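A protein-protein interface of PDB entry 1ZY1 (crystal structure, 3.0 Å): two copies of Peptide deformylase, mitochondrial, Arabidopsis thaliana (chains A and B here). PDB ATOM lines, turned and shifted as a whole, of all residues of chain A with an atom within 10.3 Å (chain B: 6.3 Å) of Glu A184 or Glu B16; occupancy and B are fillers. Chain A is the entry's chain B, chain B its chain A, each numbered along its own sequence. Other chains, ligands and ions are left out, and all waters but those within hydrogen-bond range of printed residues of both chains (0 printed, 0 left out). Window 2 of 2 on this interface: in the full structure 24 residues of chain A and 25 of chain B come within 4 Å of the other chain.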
ATOM      1  N   VAL A 168      32.733 -28.965 -10.906  1.00  0.00           N
ATOM      2  CA  VAL A 168      31.448 -29.056 -11.581  1.00  0.00           C
ATOM      3  C   VAL A 168      30.633 -27.873 -11.093  1.00  0.00           C
ATOM      4  O   VAL A 168      30.450 -27.688  -9.889  1.00  0.00           O
ATOM      5  CB  VAL A 168      30.711 -30.352 -11.214  1.00  0.00           C
ATOM      6  CG1 VAL A 168      29.350 -30.380 -11.889  1.00  0.00           C
ATOM      7  CG2 VAL A 168      31.529 -31.554 -11.640  1.00  0.00           C
ATOM      8  N   PRO A 169      30.128 -27.059 -12.020  1.00  0.00           N
ATOM      9  CA  PRO A 169      29.339 -25.886 -11.666  1.00  0.00           C
ATOM     10  C   PRO A 169      28.277 -26.191 -10.637  1.00  0.00           C
ATOM     11  O   PRO A 169      27.620 -27.228 -10.708  1.00  0.00           O
ATOM     12  CB  PRO A 169      28.733 -25.476 -12.987  1.00  0.00           C
ATOM     13  CG  PRO A 169      29.749 -25.926 -13.970  1.00  0.00           C
ATOM     14  CD  PRO A 169      30.099 -27.280 -13.468  1.00  0.00           C
ATOM     15  N   ARG A 170      28.127 -25.296  -9.668  1.00  0.00           N
ATOM     16  CA  ARG A 170      27.113 -25.442  -8.636  1.00  0.00           C
ATOM     17  C   ARG A 170      27.320 -26.527  -7.593  1.00  0.00           C
ATOM     18  O   ARG A 170      26.410 -26.806  -6.812  1.00  0.00           O
ATOM     19  CB  ARG A 170      25.752 -25.630  -9.286  1.00  0.00           C
ATOM     20  CG  ARG A 170      25.511 -24.631 -10.385  1.00  0.00           C
ATOM     21  CD  ARG A 170      24.047 -24.356 -10.605  1.00  0.00           C
ATOM     22  NE  ARG A 170      23.629 -24.524 -11.959  1.00  0.00           N
ATOM     23  CZ  ARG A 170      23.158 -23.687 -12.873  1.00  0.00           C
ATOM     24  NH1 ARG A 170      22.974 -22.384 -12.733  1.00  0.00           N
ATOM     25  NH2 ARG A 170      22.754 -24.279 -13.978  1.00  0.00           N
ATOM     26  N   THR A 171      28.494 -27.145  -7.560  1.00  0.00           N
ATOM     27  CA  THR A 171      28.722 -28.167  -6.550  1.00  0.00           C
ATOM     28  C   THR A 171      29.528 -27.561  -5.399  1.00  0.00           C
ATOM     29  O   THR A 171      29.572 -28.116  -4.301  1.00  0.00           O
ATOM     30  CB  THR A 171      29.462 -29.379  -7.138  1.00  0.00           C
ATOM     31  OG1 THR A 171      30.852 -29.061  -7.314  1.00  0.00           O
ATOM     32  CG2 THR A 171      28.865 -29.751  -8.481  1.00  0.00           C
ATOM     33  N   ARG A 173      30.703 -25.819  -2.230  1.00  0.00           N
ATOM     34  CA  ARG A 173      29.954 -25.735  -0.981  1.00  0.00           C
ATOM     35  C   ARG A 173      30.798 -25.756   0.280  1.00  0.00           C
ATOM     36  O   ARG A 173      31.966 -26.153   0.279  1.00  0.00           O
ATOM     37  CB  ARG A 173      28.961 -26.885  -0.910  1.00  0.00           C
ATOM     38  CG  ARG A 173      29.622 -28.243  -0.902  1.00  0.00           C
ATOM     39  CD  ARG A 173      28.582 -29.331  -0.945  1.00  0.00           C
ATOM     40  NE  ARG A 173      27.743 -29.189  -2.131  1.00  0.00           N
ATOM     41  CZ  ARG A 173      26.648 -29.904  -2.355  1.00  0.00           C
ATOM     42  NH1 ARG A 173      26.263 -30.813  -1.476  1.00  0.00           N
ATOM     43  NH2 ARG A 173      25.934 -29.705  -3.452  1.00  0.00           N
ATOM     44  N   LEU A 180      24.176 -31.582   1.774  1.00  0.00           N
ATOM     45  CA  LEU A 180      22.930 -31.057   1.240  1.00  0.00           C
ATOM     46  C   LEU A 180      22.828 -31.515  -0.213  1.00  0.00           C
ATOM     47  O   LEU A 180      23.846 -31.742  -0.877  1.00  0.00           O
ATOM     48  CB  LEU A 180      22.916 -29.534   1.351  1.00  0.00           C
ATOM     49  CG  LEU A 180      22.799 -29.086   2.808  1.00  0.00           C
ATOM     50  CD1 LEU A 180      23.027 -27.593   2.935  1.00  0.00           C
ATOM     51  CD2 LEU A 180      21.426 -29.450   3.328  1.00  0.00           C
ATOM     52  N   PRO A 181      21.603 -31.681  -0.726  1.00  0.00           N
ATOM     53  CA  PRO A 181      21.412 -32.123  -2.108  1.00  0.00           C
ATOM     54  C   PRO A 181      22.142 -31.311  -3.166  1.00  0.00           C
ATOM     55  O   PRO A 181      22.591 -30.202  -2.924  1.00  0.00           O
ATOM     56  CB  PRO A 181      19.898 -32.047  -2.287  1.00  0.00           C
ATOM     57  CG  PRO A 181      19.384 -32.309  -0.918  1.00  0.00           C
ATOM     58  CD  PRO A 181      20.305 -31.468  -0.068  1.00  0.00           C
ATOM     59  N   LEU A 182      22.266 -31.903  -4.345  1.00  0.00           N
ATOM     60  CA  LEU A 182      22.888 -31.240  -5.465  1.00  0.00           C
ATOM     61  C   LEU A 182      21.736 -30.531  -6.127  1.00  0.00           C
ATOM     62  O   LEU A 182      20.634 -31.071  -6.237  1.00  0.00           O
ATOM     63  CB  LEU A 182      23.488 -32.227  -6.466  1.00  0.00           C
ATOM     64  CG  LEU A 182      24.543 -33.186  -5.936  1.00  0.00           C
ATOM     65  CD1 LEU A 182      25.017 -34.074  -7.060  1.00  0.00           C
ATOM     66  CD2 LEU A 182      25.699 -32.407  -5.345  1.00  0.00           C
ATOM     67  N   ALA A 183      21.996 -29.291  -6.510  1.00  0.00           N
ATOM     68  CA  ALA A 183      20.996 -28.492  -7.190  1.00  0.00           C
ATOM     69  C   ALA A 183      20.623 -29.239  -8.451  1.00  0.00           C
ATOM     70  O   ALA A 183      21.385 -30.068  -8.943  1.00  0.00           O
ATOM     71  CB  ALA A 183      21.556 -27.112  -7.501  1.00  0.00           C
ATOM     72  N   GLU A 184      19.416 -28.970  -8.930  1.00  0.00           N
ATOM     73  CA  GLU A 184      18.946 -29.641 -10.132  1.00  0.00           C
ATOM     74  C   GLU A 184      19.729 -29.273 -11.383  1.00  0.00           C
ATOM     75  O   GLU A 184      19.999 -28.111 -11.638  1.00  0.00           O
ATOM     76  CB  GLU A 184      17.447 -29.380 -10.332  1.00  0.00           C
ATOM     77  CG  GLU A 184      17.137 -28.311 -11.355  1.00  0.00           C
ATOM     78  CD  GLU A 184      15.681 -28.382 -11.809  1.00  0.00           C
ATOM     79  OE1 GLU A 184      14.777 -27.974 -11.035  1.00  0.00           O
ATOM     80  OE2 GLU A 184      15.442 -28.860 -12.942  1.00  0.00           O
ATOM     81  N   GLY A 185      20.067 -30.290 -12.150  1.00  0.00           N
ATOM     82  CA  GLY A 185      20.825 -30.116 -13.345  1.00  0.00           C
ATOM     83  C   GLY A 185      22.181 -30.727 -13.120  1.00  0.00           C
ATOM     84  O   GLY A 185      22.787 -31.264 -14.046  1.00  0.00           O
ATOM     85  N   CYS A 186      22.654 -30.672 -11.879  1.00  0.00           N
ATOM     86  CA  CYS A 186      23.965 -31.217 -11.549  1.00  0.00           C
ATOM     87  C   CYS A 186      24.065 -32.692 -11.862  1.00  0.00           C
ATOM     88  O   CYS A 186      23.086 -33.432 -11.761  1.00  0.00           O
ATOM     89  CB  CYS A 186      24.287 -31.011 -10.073  1.00  0.00           C
ATOM     90  SG  CYS A 186      24.388 -29.290  -9.588  1.00  0.00           S
ATOM     91  N   PRO A 187      25.262 -33.138 -12.258  1.00  0.00           N
ATOM     92  CA  PRO A 187      25.502 -34.541 -12.588  1.00  0.00           C
ATOM     93  C   PRO A 187      25.280 -35.391 -11.340  1.00  0.00           C
ATOM     94  O   PRO A 187      25.066 -34.855 -10.256  1.00  0.00           O
ATOM     95  CB  PRO A 187      26.968 -34.542 -13.023  1.00  0.00           C
ATOM     96  CG  PRO A 187      27.154 -33.173 -13.617  1.00  0.00           C
ATOM     97  CD  PRO A 187      26.430 -32.310 -12.609  1.00  0.00           C
ATOM     98  N   LYS A 188      25.319 -36.712 -11.493  1.00  0.00           N
ATOM     99  CA  LYS A 188      25.154 -37.625 -10.361  1.00  0.00           C
ATOM    100  C   LYS A 188      26.566 -38.045  -9.941  1.00  0.00           C
ATOM    101  O   LYS A 188      27.408 -38.301 -10.800  1.00  0.00           O
ATOM    102  CB  LYS A 188      24.326 -38.852 -10.783  1.00  0.00           C
ATOM    103  N   ASP B  11      23.679 -25.161  -0.056  1.00  0.00           N
ATOM    104  CA  ASP B  11      22.232 -25.091   0.098  1.00  0.00           C
ATOM    105  C   ASP B  11      21.605 -24.889  -1.273  1.00  0.00           C
ATOM    106  O   ASP B  11      21.720 -23.816  -1.859  1.00  0.00           O
ATOM    107  CB  ASP B  11      21.866 -23.929   1.014  1.00  0.00           C
ATOM    108  CG  ASP B  11      20.427 -23.967   1.448  1.00  0.00           C
ATOM    109  OD1 ASP B  11      19.539 -24.114   0.577  1.00  0.00           O
ATOM    110  OD2 ASP B  11      20.187 -23.845   2.664  1.00  0.00           O
ATOM    111  N   PRO B  12      20.911 -25.911  -1.792  1.00  0.00           N
ATOM    112  CA  PRO B  12      20.255 -25.894  -3.103  1.00  0.00           C
ATOM    113  C   PRO B  12      19.600 -24.581  -3.505  1.00  0.00           C
ATOM    114  O   PRO B  12      19.596 -24.212  -4.673  1.00  0.00           O
ATOM    115  CB  PRO B  12      19.241 -27.027  -2.986  1.00  0.00           C
ATOM    116  CG  PRO B  12      19.953 -27.994  -2.128  1.00  0.00           C
ATOM    117  CD  PRO B  12      20.498 -27.105  -1.037  1.00  0.00           C
ATOM    118  N   VAL B  13      19.056 -23.873  -2.529  1.00  0.00           N
ATOM    119  CA  VAL B  13      18.378 -22.620  -2.806  1.00  0.00           C
ATOM    120  C   VAL B  13      19.248 -21.659  -3.607  1.00  0.00           C
ATOM    121  O   VAL B  13      18.741 -20.879  -4.404  1.00  0.00           O
ATOM    122  CB  VAL B  13      17.934 -21.938  -1.497  1.00  0.00           C
ATOM    123  CG1 VAL B  13      19.150 -21.469  -0.719  1.00  0.00           C
ATOM    124  CG2 VAL B  13      16.988 -20.790  -1.798  1.00  0.00           C
ATOM    125  N   LEU B  14      20.558 -21.721  -3.400  1.00  0.00           N
ATOM    126  CA  LEU B  14      21.484 -20.841  -4.114  1.00  0.00           C
ATOM    127  C   LEU B  14      21.894 -21.311  -5.497  1.00  0.00           C
ATOM    128  O   LEU B  14      22.390 -20.516  -6.290  1.00  0.00           O
ATOM    129  CB  LEU B  14      22.775 -20.626  -3.326  1.00  0.00           C
ATOM    130  CG  LEU B  14      22.664 -19.860  -2.023  1.00  0.00           C
ATOM    131  CD1 LEU B  14      22.341 -20.834  -0.924  1.00  0.00           C
ATOM    132  CD2 LEU B  14      23.965 -19.158  -1.718  1.00  0.00           C
ATOM    133  N   HIS B  15      21.713 -22.596  -5.783  1.00  0.00           N
ATOM    134  CA  HIS B  15      22.128 -23.120  -7.071  1.00  0.00           C
ATOM    135  C   HIS B  15      20.980 -23.540  -7.964  1.00  0.00           C
ATOM    136  O   HIS B  15      21.141 -24.404  -8.823  1.00  0.00           O
ATOM    137  CB  HIS B  15      23.095 -24.285  -6.867  1.00  0.00           C
ATOM    138  CG  HIS B  15      24.167 -24.009  -5.868  1.00  0.00           C
ATOM    139  ND1 HIS B  15      24.036 -24.299  -4.517  1.00  0.00           N
ATOM    140  CD2 HIS B  15      25.400 -23.451  -5.987  1.00  0.00           C
ATOM    141  CE1 HIS B  15      25.117 -23.942  -3.871  1.00  0.00           C
ATOM    142  NE2 HIS B  15      25.972 -23.417  -4.749  1.00  0.00           N
ATOM    143  N   GLU B  16      19.824 -22.914  -7.762  1.00  0.00           N
ATOM    144  CA  GLU B  16      18.636 -23.200  -8.560  1.00  0.00           C
ATOM    145  C   GLU B  16      17.934 -21.899  -8.944  1.00  0.00           C
ATOM    146  O   GLU B  16      17.899 -20.946  -8.168  1.00  0.00           O
ATOM    147  CB  GLU B  16      17.664 -24.105  -7.791  1.00  0.00           C
ATOM    148  CG  GLU B  16      18.286 -25.405  -7.291  1.00  0.00           C
ATOM    149  CD  GLU B  16      17.278 -26.369  -6.681  1.00  0.00           C
ATOM    150  OE1 GLU B  16      16.425 -25.928  -5.878  1.00  0.00           O
ATOM    151  OE2 GLU B  16      17.357 -27.578  -6.995  1.00  0.00           O
ATOM    152  N   LYS B  17      17.379 -21.866 -10.150  1.00  0.00           N
ATOM    153  CA  LYS B  17      16.688 -20.683 -10.650  1.00  0.00           C
ATOM    154  C   LYS B  17      15.517 -20.309  -9.748  1.00  0.00           C
ATOM    155  O   LYS B  17      14.664 -21.145  -9.455  1.00  0.00           O
ATOM    156  CB  LYS B  17      16.206 -20.943 -12.076  1.00  0.00           C
ATOM    157  CG  LYS B  17      15.658 -19.721 -12.765  1.00  0.00           C
ATOM    158  CD  LYS B  17      15.409 -19.992 -14.236  1.00  0.00           C
ATOM    159  CE  LYS B  17      15.188 -18.684 -14.982  1.00  0.00           C
ATOM    160  NZ  LYS B  17      14.560 -18.860 -16.321  1.00  0.00           N
ATOM    161  N   ALA B  18      15.487 -19.049  -9.314  1.00  0.00           N
ATOM    162  CA  ALA B  18      14.428 -18.560  -8.427  1.00  0.00           C
ATOM    163  C   ALA B  18      13.166 -18.155  -9.173  1.00  0.00           C
ATOM    164  O   ALA B  18      13.216 -17.556 -10.242  1.00  0.00           O
ATOM    165  CB  ALA B  18      14.929 -17.398  -7.596  1.00  0.00           C
ATOM    166  N   PRO B  53      17.493 -15.578  -2.687  1.00  0.00           N
ATOM    167  CA  PRO B  53      17.964 -16.917  -2.333  1.00  0.00           C
ATOM    168  C   PRO B  53      18.984 -16.913  -1.223  1.00  0.00           C
ATOM    169  O   PRO B  53      19.072 -17.869  -0.474  1.00  0.00           O
ATOM    170  CB  PRO B  53      18.544 -17.435  -3.640  1.00  0.00           C
ATOM    171  CG  PRO B  53      17.637 -16.826  -4.650  1.00  0.00           C
ATOM    172  CD  PRO B  53      17.502 -15.395  -4.145  1.00  0.00           C
ATOM    173  N   HIS B 157      22.711 -14.827  -8.979  1.00  0.00           N
ATOM    174  CA  HIS B 157      22.152 -15.548  -7.843  1.00  0.00           C
ATOM    175  C   HIS B 157      20.746 -16.032  -8.143  1.00  0.00           C
ATOM    176  O   HIS B 157      20.400 -17.171  -7.854  1.00  0.00           O
ATOM    177  CB  HIS B 157      22.109 -14.643  -6.611  1.00  0.00           C
ATOM    178  CG  HIS B 157      23.428 -14.553  -5.882  1.00  0.00           C
ATOM    179  ND1 HIS B 157      23.885 -15.554  -5.076  1.00  0.00           N
ATOM    180  CD2 HIS B 157      24.375 -13.588  -5.897  1.00  0.00           C
ATOM    181  CE1 HIS B 157      25.088 -15.213  -4.607  1.00  0.00           C
ATOM    182  NE2 HIS B 157      25.401 -14.040  -5.086  1.00  0.00           N
ATOM    183  N   LEU B 158      19.933 -15.152  -8.720  1.00  0.00           N
ATOM    184  CA  LEU B 158      18.556 -15.490  -9.045  1.00  0.00           C
ATOM    185  C   LEU B 158      18.477 -16.638 -10.039  1.00  0.00           C
ATOM    186  O   LEU B 158      17.401 -17.169 -10.294  1.00  0.00           O
ATOM    187  CB  LEU B 158      17.819 -14.258  -9.587  1.00  0.00           C
ATOM    188  CG  LEU B 158      17.842 -12.993  -8.723  1.00  0.00           C
ATOM    189  CD1 LEU B 158      16.962 -11.939  -9.364  1.00  0.00           C
ATOM    190  CD2 LEU B 158      17.352 -13.297  -7.318  1.00  0.00           C
ATOM    191  N   ASP B 159      19.614 -17.024 -10.603  1.00  0.00           N
ATOM    192  CA  ASP B 159      19.627 -18.139 -11.538  1.00  0.00           C
ATOM    193  C   ASP B 159      20.405 -19.354 -11.063  1.00  0.00           C
ATOM    194  O   ASP B 159      20.571 -20.319 -11.809  1.00  0.00           O
ATOM    195  CB  ASP B 159      20.163 -17.717 -12.890  1.00  0.00           C
ATOM    196  CG  ASP B 159      19.118 -17.035 -13.717  1.00  0.00           C
ATOM    197  OD1 ASP B 159      17.944 -17.411 -13.576  1.00  0.00           O
ATOM    198  OD2 ASP B 159      19.462 -16.141 -14.515  1.00  0.00           O
ATOM    199  N   GLY B 160      20.864 -19.310  -9.817  1.00  0.00           N
ATOM    200  CA  GLY B 160      21.616 -20.422  -9.261  1.00  0.00           C
ATOM    201  C   GLY B 160      23.081 -20.409  -9.639  1.00  0.00           C
ATOM    202  O   GLY B 160      23.729 -21.453  -9.693  1.00  0.00           O
ATOM    203  N   ASN B 161      23.611 -19.219  -9.877  1.00  0.00           N
ATOM    204  CA  ASN B 161      24.999 -19.083 -10.266  1.00  0.00           C
ATOM    205  C   ASN B 161      25.821 -18.213  -9.354  1.00  0.00           C
ATOM    206  O   ASN B 161      25.432 -17.094  -9.045  1.00  0.00           O
ATOM    207  CB  ASN B 161      25.074 -18.529 -11.675  1.00  0.00           C
ATOM    208  CG  ASN B 161      24.309 -19.373 -12.650  1.00  0.00           C
ATOM    209  OD1 ASN B 161      24.510 -20.587 -12.715  1.00  0.00           O
ATOM    210  ND2 ASN B 161      23.423 -18.742 -13.423  1.00  0.00           N
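The guanidinium group (NH2) of Arg A173 sits at hydrogen-bond distance from the backbone carbonyl oxygen (O) of Pro A181.
OD1 of Asp B11 lies close to N of Val B13 (3.2 Å).
The backbone carbonyl oxygen (O) of Ala A183 is in hydrogen-bond range of the side-chain sulfur (SG) of Cys A186, at 3.2 Å.
The guanidinium group (NH1) of Arg A173 lies within hydrogen-bond range of the backbone carbonyl oxygen (O) of Leu A180.
No position is printed for both chains.
Of the 9 pairs that touch across the chains among the printed residues, none has its exchanged pair printed and touching as well.
Glu A184 touches one residue of chain B.
Of chain A, only Ala A183 and Glu A184 come within 4 Å of Glu B16.
No residue of chain A comes within 4 Å of Ala B18.
Gly B160 touches one residue of chain A.
Of the printed residues of chain B, Arg A170 touches His B15, Asp B159, Gly B160 and Asn B161.
Of the printed residues of chain A, Pro B12 touches Pro A181.
Of the printed residues of chain A, Asp B159 touches Arg A170.
Of the printed residues of chain B, Pro A181 touches Pro B12.
Pro A187 touches none of the printed residues of chain B.
N of Glu A184 is in hydrogen-bond range of OE2 of Glu B16, at 3.1 Å.
The guanidinium group of Arg A170 sits at hydrogen-bond distance from the backbone carbonyl oxygen of Asp B159 (3.3 Å).
The backbone carbonyl oxygen of Gly B160 lies close to the guanidinium group of Arg A170 (3.3 Å).
The guanidinium group of Arg A170 sits close to the side-chain amide oxygen of Asn B161 (2.4 Å).
Of the 14 printed residues of chain A, 5 touch a printed residue of chain B.
Among the printed residues, no Asp or Glu carboxylate lies within 4 Å of a Lys or Arg side-chain nitrogen of the other chain.
Among the printed residues, pairs that only touch across the chains: Ala A183 with His B15, Arg A170 with His B15, Pro A181 with Pro B12, Ala A183 with Glu B16 and Leu A180 with Asp B11.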
